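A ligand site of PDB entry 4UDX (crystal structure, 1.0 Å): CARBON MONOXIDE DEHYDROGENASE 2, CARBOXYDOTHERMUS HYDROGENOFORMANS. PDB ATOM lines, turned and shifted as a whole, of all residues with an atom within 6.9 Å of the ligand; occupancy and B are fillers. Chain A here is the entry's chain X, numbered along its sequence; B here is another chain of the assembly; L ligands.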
ATOM      1  N   CYS A  47     -15.782 -21.558 -22.879  1.00  0.00           N
ATOM      2  CA  CYS A  47     -16.144 -20.877 -21.660  1.00  0.00           C
ATOM      3  C   CYS A  47     -17.239 -21.697 -20.981  1.00  0.00           C
ATOM      4  O   CYS A  47     -18.136 -22.220 -21.654  1.00  0.00           O
ATOM      5  CB  CYS A  47     -16.598 -19.453 -21.906  1.00  0.00           C
ATOM      6  SG  CYS A  47     -17.091 -18.611 -20.349  1.00  0.00           S
ATOM      7  N   CYS A  48     -17.127 -21.813 -19.662  1.00  0.00           N
ATOM      8  CA  CYS A  48     -18.103 -22.496 -18.833  1.00  0.00           C
ATOM      9  C   CYS A  48     -18.398 -21.660 -17.580  1.00  0.00           C
ATOM     10  O   CYS A  48     -17.493 -21.246 -16.869  1.00  0.00           O
ATOM     11  CB  CYS A  48     -17.606 -23.885 -18.439  1.00  0.00           C
ATOM     12  SG  CYS A  48     -18.806 -24.835 -17.458  1.00  0.00           S
ATOM     13  N   ARG A  49     -19.696 -21.513 -17.313  1.00  0.00           N
ATOM     14  CA  ARG A  49     -20.225 -20.876 -16.116  1.00  0.00           C
ATOM     15  C   ARG A  49     -21.222 -21.764 -15.422  1.00  0.00           C
ATOM     16  O   ARG A  49     -22.152 -21.301 -14.762  1.00  0.00           O
ATOM     17  CB  ARG A  49     -20.826 -19.502 -16.444  1.00  0.00           C
ATOM     18  CG  ARG A  49     -19.838 -18.569 -17.048  1.00  0.00           C
ATOM     19  CD  ARG A  49     -20.508 -17.331 -17.616  1.00  0.00           C
ATOM     20  NE  ARG A  49     -21.309 -16.666 -16.656  1.00  0.00           N
ATOM     21  CZ  ARG A  49     -22.332 -15.892 -16.855  1.00  0.00           C
ATOM     22  NH1 ARG A  49     -22.718 -15.562 -18.084  1.00  0.00           N
ATOM     23  NH2 ARG A  49     -22.969 -15.340 -15.806  1.00  0.00           N
ATOM     24  N   HIS A  50     -21.030 -23.088 -15.521  1.00  0.00           N
ATOM     25  CA  HIS A  50     -21.961 -24.052 -14.927  1.00  0.00           C
ATOM     26  C   HIS A  50     -21.832 -24.229 -13.423  1.00  0.00           C
ATOM     27  O   HIS A  50     -22.643 -24.929 -12.845  1.00  0.00           O
ATOM     28  CB  HIS A  50     -21.976 -25.367 -15.651  1.00  0.00           C
ATOM     29  CG  HIS A  50     -22.476 -25.277 -17.072  1.00  0.00           C
ATOM     30  ND1 HIS A  50     -22.838 -26.392 -17.780  1.00  0.00           N
ATOM     31  CD2 HIS A  50     -22.635 -24.226 -17.932  1.00  0.00           C
ATOM     32  CE1 HIS A  50     -23.200 -25.995 -19.022  1.00  0.00           C
ATOM     33  NE2 HIS A  50     -23.103 -24.705 -19.156  1.00  0.00           N
ATOM     34  N   CYS A  51     -20.884 -23.587 -12.759  1.00  0.00           N
ATOM     35  CA  CYS A  51     -20.876 -23.585 -11.311  1.00  0.00           C
ATOM     36  C   CYS A  51     -20.199 -22.311 -10.826  1.00  0.00           C
ATOM     37  O   CYS A  51     -19.620 -21.541 -11.598  1.00  0.00           O
ATOM     38  CB  CYS A  51     -20.249 -24.839 -10.688  1.00  0.00           C
ATOM     39  SG  CYS A  51     -18.419 -24.831 -10.651  1.00  0.00           S
ATOM     40  N   LEU A  52     -20.254 -22.102  -9.513  1.00  0.00           N
ATOM     41  CA  LEU A  52     -19.737 -20.891  -8.897  1.00  0.00           C
ATOM     42  C   LEU A  52     -18.233 -20.890  -8.650  1.00  0.00           C
ATOM     43  O   LEU A  52     -17.691 -19.936  -8.105  1.00  0.00           O
ATOM     44  CB  LEU A  52     -20.508 -20.574  -7.592  1.00  0.00           C
ATOM     45  CG  LEU A  52     -21.993 -20.392  -7.738  1.00  0.00           C
ATOM     46  CD1 LEU A  52     -22.577 -20.084  -6.363  1.00  0.00           C
ATOM     47  CD2 LEU A  52     -22.362 -19.295  -8.744  1.00  0.00           C
ATOM     48  N   GLN A  53     -17.548 -21.963  -9.100  1.00  0.00           N
ATOM     49  CA  GLN A  53     -16.103 -21.906  -9.208  1.00  0.00           C
ATOM     50  C   GLN A  53     -15.637 -21.167 -10.462  1.00  0.00           C
ATOM     51  O   GLN A  53     -14.516 -20.711 -10.526  1.00  0.00           O
ATOM     52  CB  GLN A  53     -15.457 -23.274  -9.173  1.00  0.00           C
ATOM     53  CG  GLN A  53     -15.626 -23.931  -7.836  1.00  0.00           C
ATOM     54  CD  GLN A  53     -15.095 -25.303  -7.654  1.00  0.00           C
ATOM     55  OE1 GLN A  53     -14.968 -26.081  -8.652  1.00  0.00           O
ATOM     56  NE2 GLN A  53     -14.759 -25.739  -6.542  1.00  0.00           N
ATOM     57  N   GLY A  54     -16.539 -21.075 -11.459  1.00  0.00           N
ATOM     58  CA  GLY A  54     -16.242 -20.368 -12.663  1.00  0.00           C
ATOM     59  C   GLY A  54     -16.310 -18.874 -12.483  1.00  0.00           C
ATOM     60  O   GLY A  54     -16.459 -18.340 -11.372  1.00  0.00           O
ATOM     61  N   PRO A  55     -16.166 -18.100 -13.556  1.00  0.00           N
ATOM     62  CA  PRO A  55     -16.100 -18.620 -14.965  1.00  0.00           C
ATOM     63  C   PRO A  55     -14.792 -19.302 -15.307  1.00  0.00           C
ATOM     64  O   PRO A  55     -13.723 -18.855 -14.857  1.00  0.00           O
ATOM     65  CB  PRO A  55     -16.284 -17.328 -15.757  1.00  0.00           C
ATOM     66  CG  PRO A  55     -15.704 -16.264 -14.878  1.00  0.00           C
ATOM     67  CD  PRO A  55     -16.115 -16.639 -13.496  1.00  0.00           C
ATOM     68  N   CYS A  56     -14.892 -20.393 -16.034  1.00  0.00           N
ATOM     69  CA  CYS A  56     -13.754 -21.093 -16.565  1.00  0.00           C
ATOM     70  C   CYS A  56     -13.645 -20.832 -18.050  1.00  0.00           C
ATOM     71  O   CYS A  56     -14.664 -20.694 -18.735  1.00  0.00           O
ATOM     72  CB  CYS A  56     -13.851 -22.594 -16.339  1.00  0.00           C
ATOM     73  SG  CYS A  56     -13.668 -23.025 -14.551  1.00  0.00           S
ATOM     74  N   ARG A  57     -12.447 -20.831 -18.577  1.00  0.00           N
ATOM     75  CA  ARG A  57     -12.180 -20.713 -19.994  1.00  0.00           C
ATOM     76  C   ARG A  57     -10.989 -21.609 -20.309  1.00  0.00           C
ATOM     77  O   ARG A  57     -10.216 -21.993 -19.430  1.00  0.00           O
ATOM     78  CB  ARG A  57     -11.902 -19.258 -20.399  1.00  0.00           C
ATOM     79  CG  ARG A  57     -10.584 -18.745 -19.855  1.00  0.00           C
ATOM     80  CD  ARG A  57     -10.497 -17.215 -19.797  1.00  0.00           C
ATOM     81  NE  ARG A  57      -9.142 -16.850 -19.392  1.00  0.00           N
ATOM     82  CZ  ARG A  57      -8.697 -16.965 -18.158  1.00  0.00           C
ATOM     83  NH1 ARG A  57      -9.478 -17.293 -17.117  1.00  0.00           N
ATOM     84  NH2 ARG A  57      -7.421 -16.688 -17.895  1.00  0.00           N
ATOM     85  N   VAL A  67      -7.801 -26.531 -19.226  1.00  0.00           N
ATOM     86  CA  VAL A  67      -8.819 -27.375 -18.644  1.00  0.00           C
ATOM     87  C   VAL A  67      -9.623 -26.593 -17.647  1.00  0.00           C
ATOM     88  O   VAL A  67      -9.101 -25.681 -17.000  1.00  0.00           O
ATOM     89  CB  VAL A  67      -8.161 -28.640 -18.033  1.00  0.00           C
ATOM     90  CG1 VAL A  67      -7.187 -28.292 -16.949  1.00  0.00           C
ATOM     91  CG2 VAL A  67      -9.149 -29.662 -17.634  1.00  0.00           C
ATOM     92  N   GLY A  68     -10.900 -26.900 -17.499  1.00  0.00           N
ATOM     93  CA  GLY A  68     -11.702 -26.289 -16.461  1.00  0.00           C
ATOM     94  C   GLY A  68     -11.246 -26.654 -15.072  1.00  0.00           C
ATOM     95  O   GLY A  68     -10.567 -27.631 -14.836  1.00  0.00           O
ATOM     96  N   ILE A  69     -11.704 -25.860 -14.085  1.00  0.00           N
ATOM     97  CA  ILE A  69     -11.257 -26.077 -12.717  1.00  0.00           C
ATOM     98  C   ILE A  69     -11.628 -27.466 -12.192  1.00  0.00           C
ATOM     99  O   ILE A  69     -10.837 -28.085 -11.506  1.00  0.00           O
ATOM    100  CB  ILE A  69     -11.787 -24.949 -11.800  1.00  0.00           C
ATOM    101  CG1 ILE A  69     -11.090 -23.637 -12.123  1.00  0.00           C
ATOM    102  CG2 ILE A  69     -11.672 -25.300 -10.312  1.00  0.00           C
ATOM    103  CD1 ILE A  69     -11.692 -22.408 -11.515  1.00  0.00           C
ATOM    104  N   CYS A  70     -12.822 -27.961 -12.533  1.00  0.00           N
ATOM    105  CA  CYS A  70     -13.257 -29.309 -12.093  1.00  0.00           C
ATOM    106  C   CYS A  70     -12.611 -30.427 -12.906  1.00  0.00           C
ATOM    107  O   CYS A  70     -12.861 -31.607 -12.593  1.00  0.00           O
ATOM    108  CB  CYS A  70     -14.784 -29.430 -12.203  1.00  0.00           C
ATOM    109  SG  CYS A  70     -15.332 -29.202 -13.925  1.00  0.00           S
ATOM    110  N   GLY A  71     -11.845 -30.077 -13.937  1.00  0.00           N
ATOM    111  CA  GLY A  71     -11.290 -31.063 -14.835  1.00  0.00           C
ATOM    112  C   GLY A  71     -12.017 -31.178 -16.185  1.00  0.00           C
ATOM    113  O   GLY A  71     -11.665 -32.004 -17.012  1.00  0.00           O
ATOM    114  N   ALA A  72     -13.055 -30.370 -16.402  1.00  0.00           N
ATOM    115  CA  ALA A  72     -13.810 -30.410 -17.657  1.00  0.00           C
ATOM    116  C   ALA A  72     -12.890 -30.057 -18.817  1.00  0.00           C
ATOM    117  O   ALA A  72     -12.314 -28.956 -18.838  1.00  0.00           O
ATOM    118  CB  ALA A  72     -15.018 -29.499 -17.584  1.00  0.00           C
ATOM    119  N   THR A  73     -12.833 -30.928 -19.809  1.00  0.00           N
ATOM    120  CA  THR A  73     -12.037 -30.681 -20.989  1.00  0.00           C
ATOM    121  C   THR A  73     -12.729 -29.768 -21.973  1.00  0.00           C
ATOM    122  O   THR A  73     -13.916 -29.476 -21.871  1.00  0.00           O
ATOM    123  CB  THR A  73     -11.705 -32.000 -21.705  1.00  0.00           C
ATOM    124  OG1 THR A  73     -12.954 -32.519 -22.134  1.00  0.00           O
ATOM    125  CG2 THR A  73     -10.942 -32.984 -20.843  1.00  0.00           C
ATOM    126  N   ILE A  77     -16.775 -29.128 -22.246  1.00  0.00           N
ATOM    127  CA  ILE A  77     -17.319 -27.809 -22.142  1.00  0.00           C
ATOM    128  C   ILE A  77     -18.119 -27.422 -23.415  1.00  0.00           C
ATOM    129  O   ILE A  77     -19.236 -26.938 -23.338  1.00  0.00           O
ATOM    130  CB  ILE A  77     -16.232 -26.740 -21.793  1.00  0.00           C
ATOM    131  CG1 ILE A  77     -15.768 -26.966 -20.342  1.00  0.00           C
ATOM    132  CG2 ILE A  77     -16.655 -25.341 -22.123  1.00  0.00           C
ATOM    133  CD1 ILE A  77     -14.542 -26.116 -20.005  1.00  0.00           C
ATOM    134  N   ARG A  80     -21.328 -29.556 -23.626  1.00  0.00           N
ATOM    135  CA  ARG A  80     -22.345 -29.156 -22.645  1.00  0.00           C
ATOM    136  C   ARG A  80     -23.049 -27.874 -23.040  1.00  0.00           C
ATOM    137  O   ARG A  80     -24.261 -27.732 -22.899  1.00  0.00           O
ATOM    138  CB  ARG A  80     -21.728 -29.045 -21.224  1.00  0.00           C
ATOM    139  CG  ARG A  80     -21.236 -30.347 -20.671  1.00  0.00           C
ATOM    140  CD  ARG A  80     -20.913 -30.312 -19.180  1.00  0.00           C
ATOM    141  NE  ARG A  80     -19.935 -29.252 -18.869  1.00  0.00           N
ATOM    142  CZ  ARG A  80     -19.277 -29.177 -17.712  1.00  0.00           C
ATOM    143  NH1 ARG A  80     -19.458 -30.106 -16.811  1.00  0.00           N
ATOM    144  NH2 ARG A  80     -18.432 -28.185 -17.461  1.00  0.00           N
ATOM    145  N   THR A 197     -25.645 -31.854 -18.044  1.00  0.00           N
ATOM    146  CA  THR A 197     -24.693 -30.800 -18.364  1.00  0.00           C
ATOM    147  C   THR A 197     -24.313 -29.967 -17.133  1.00  0.00           C
ATOM    148  O   THR A 197     -23.426 -29.099 -17.251  1.00  0.00           O
ATOM    149  CB  THR A 197     -25.210 -29.879 -19.475  1.00  0.00           C
ATOM    150  OG1 THR A 197     -26.448 -29.315 -19.046  1.00  0.00           O
ATOM    151  CG2 THR A 197     -25.415 -30.608 -20.786  1.00  0.00           C
ATOM    152  N   SER A 198     -24.960 -30.206 -15.996  1.00  0.00           N
ATOM    153  CA  SER A 198     -24.567 -29.512 -14.757  1.00  0.00           C
ATOM    154  C   SER A 198     -23.243 -30.068 -14.268  1.00  0.00           C
ATOM    155  O   SER A 198     -22.739 -31.097 -14.737  1.00  0.00           O
ATOM    156  CB  SER A 198     -25.685 -29.627 -13.737  1.00  0.00           C
ATOM    157  OG  SER A 198     -25.815 -30.868 -13.111  1.00  0.00           O
ATOM    158  N   MET A 199     -22.641 -29.390 -13.317  1.00  0.00           N
ATOM    159  CA  MET A 199     -21.302 -29.747 -12.867  1.00  0.00           C
ATOM    160  C   MET A 199     -21.248 -31.162 -12.332  1.00  0.00           C
ATOM    161  O   MET A 199     -22.106 -31.641 -11.571  1.00  0.00           O
ATOM    162  CB  MET A 199     -20.766 -28.691 -11.893  1.00  0.00           C
ATOM    163  CG  MET A 199     -19.375 -28.951 -11.365  1.00  0.00           C
ATOM    164  SD  MET A 199     -19.347 -30.164 -10.006  1.00  0.00           S
ATOM    165  CE  MET A 199     -17.700 -30.746 -10.121  1.00  0.00           C
ATOM    166  N   GLY A 200     -20.192 -31.869 -12.764  1.00  0.00           N
ATOM    167  CA  GLY A 200     -19.907 -33.152 -12.189  1.00  0.00           C
ATOM    168  C   GLY A 200     -20.825 -34.285 -12.635  1.00  0.00           C
ATOM    169  O   GLY A 200     -20.931 -35.280 -11.902  1.00  0.00           O
ATOM    170  N   VAL B  28      -7.430 -29.844  -8.299  1.00  0.00           N
ATOM    171  CA  VAL B  28      -8.390 -28.738  -8.487  1.00  0.00           C
ATOM    172  C   VAL B  28      -7.821 -27.398  -8.105  1.00  0.00           C
ATOM    173  O   VAL B  28      -8.090 -26.383  -8.781  1.00  0.00           O
ATOM    174  CB  VAL B  28      -9.691 -29.068  -7.693  1.00  0.00           C
ATOM    175  CG1 VAL B  28      -9.440 -29.139  -6.192  1.00  0.00           C
ATOM    176  CG2 VAL B  28     -10.782 -28.084  -8.039  1.00  0.00           C
ATOM    177  N   MET B  35      -6.319 -20.804 -13.846  1.00  0.00           N
ATOM    178  CA  MET B  35      -7.433 -20.051 -14.394  1.00  0.00           C
ATOM    179  C   MET B  35      -7.388 -18.563 -14.038  1.00  0.00           C
ATOM    180  O   MET B  35      -8.153 -17.772 -14.629  1.00  0.00           O
ATOM    181  CB  MET B  35      -8.733 -20.691 -13.852  1.00  0.00           C
ATOM    182  CG  MET B  35      -9.987 -20.342 -14.648  1.00  0.00           C
ATOM    183  SD  MET B  35      -9.873 -20.905 -16.394  1.00  0.00           S
ATOM    184  CE  MET B  35      -9.982 -22.670 -16.177  1.00  0.00           C
ATOM    185  N   GLN B  38      -9.680 -14.778 -13.373  1.00  0.00           N
ATOM    186  CA  GLN B  38     -10.936 -15.184 -14.007  1.00  0.00           C
ATOM    187  C   GLN B  38     -11.618 -13.983 -14.673  1.00  0.00           C
ATOM    188  O   GLN B  38     -11.440 -12.851 -14.270  1.00  0.00           O
ATOM    189  CB  GLN B  38     -11.845 -15.916 -13.013  1.00  0.00           C
ATOM    190  CG  GLN B  38     -11.270 -17.235 -12.580  1.00  0.00           C
ATOM    191  CD  GLN B  38     -12.116 -17.967 -11.574  1.00  0.00           C
ATOM    192  OE1 GLN B  38     -12.111 -17.656 -10.383  1.00  0.00           O
ATOM    193  NE2 GLN B  38     -12.867 -18.927 -12.066  1.00  0.00           N
ATOM    194  N   PRO B 336     -14.554 -34.379 -13.107  1.00  0.00           N
ATOM    195  CA  PRO B 336     -14.178 -35.376 -14.121  1.00  0.00           C
ATOM    196  C   PRO B 336     -12.707 -35.625 -14.169  1.00  0.00           C
ATOM    197  O   PRO B 336     -12.246 -36.631 -14.755  1.00  0.00           O
ATOM    198  CB  PRO B 336     -14.727 -34.791 -15.412  1.00  0.00           C
ATOM    199  CG  PRO B 336     -14.865 -33.306 -15.153  1.00  0.00           C
ATOM    200  CD  PRO B 336     -15.258 -33.218 -13.693  1.00  0.00           C
ATOM    201  N   MET B 560     -21.146 -23.915  -4.467  1.00  0.00           N
ATOM    202  CA  MET B 560     -20.545 -24.202  -5.781  1.00  0.00           C
ATOM    203  C   MET B 560     -21.584 -24.558  -6.840  1.00  0.00           C
ATOM    204  O   MET B 560     -21.640 -23.913  -7.892  1.00  0.00           O
ATOM    205  CB  MET B 560     -19.465 -25.294  -5.633  1.00  0.00           C
ATOM    206  CG  MET B 560     -18.757 -25.727  -6.910  1.00  0.00           C
ATOM    207  SD  MET B 560     -19.531 -27.077  -7.810  1.00  0.00           S
ATOM    208  CE  MET B 560     -19.476 -28.395  -6.621  1.00  0.00           C
HETATM  209 FE1  LIG L   1     -17.666 -25.130 -12.773  1.00  0.00          FE
HETATM  210 FE2  LIG L   1     -17.687 -25.221 -15.499  1.00  0.00          FE
HETATM  211 FE3  LIG L   1     -15.477 -24.430 -14.221  1.00  0.00          FE
HETATM  212 FE4  LIG L   1     -16.204 -27.072 -14.143  1.00  0.00          FE
HETATM  213  S1  LIG L   1     -15.536 -25.942 -16.005  1.00  0.00           S
HETATM  214  S2  LIG L   1     -15.423 -25.733 -12.375  1.00  0.00           S
HETATM  215  S3  LIG L   1     -18.526 -26.825 -14.135  1.00  0.00           S
HETATM  216  S4  LIG L   1     -17.532 -23.333 -14.181  1.00  0.00           S
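SG of Cys 48 binds FE2 of the ligand, at 2.3 Å. N of His 50 sits close to S4 of the ligand. The backbone NH (N) of Cys 51 lies close to a sulfur (S4) of the ligand (3.7 Å). A sulfur (S4) of the ligand lies close to the backbone NH (N) of Gly 54 (3.7 Å). OE1 of Gln 53 sits close to S2 of the ligand, at 3.8 Å. The side-chain sulfur (SG) of Cys 51 is bound to an iron atom (FE1) of the ligand (2.3 Å). The guanidinium group (NH2) of Arg 80 lies close to a sulfur (S3) of the ligand, at 3.6 Å. SG of Cys 56 is bound to FE3 of the ligand (2.3 Å). The backbone NH (N) of Cys 70 lies close to a sulfur (S2) of the ligand (3.4 Å). SG of Cys 70 is bound to FE4 of the ligand, 2.3 Å away.
A ring nitrogen (ND1) of His 50 is in hydrogen-bond range of the backbone carbonyl oxygen (O) of Thr 197, at 2.8 Å. N of His 50 lies close to SG of Cys 48, 3.4 Å away. SG of Cys 51 sits close to SD of Met 560 of chain B. NH2 of Arg 80 sits close to SG of Cys 48. SG of Cys 56 lies close to N of Ile 69 (3.5 Å). The backbone carbonyl oxygen (O) of Gln 53 sits at hydrogen-bond distance from the side-chain amide nitrogen (NE2) of Gln 38 of chain B (2.9 Å). The backbone carbonyl oxygen (O) of Cys 56 sits close to the side-chain sulfur (SG) of Cys 47 (3.6 Å). O of Cys 56 lies within hydrogen-bond range of N of Cys 48 (2.9 Å).
Gly 68 touches the ligand (CA to S1, 3.9 Å). Ile 69 touches the ligand. CB of Ala 72 touches S1 of the ligand, at 3.9 Å. Met 199 touches the ligand (CG to S3, 3.6 Å). Within 4 Å of the ligand: Cys 48, His 50, Cys 51, Gln 53, Gly 54, Cys 56, Gly 68, Ile 69, Cys 70, Ala 72, Arg 80 and Met 199. The nearest printed residue that does not touch the ligand is Ile 77 (4.1 Å).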
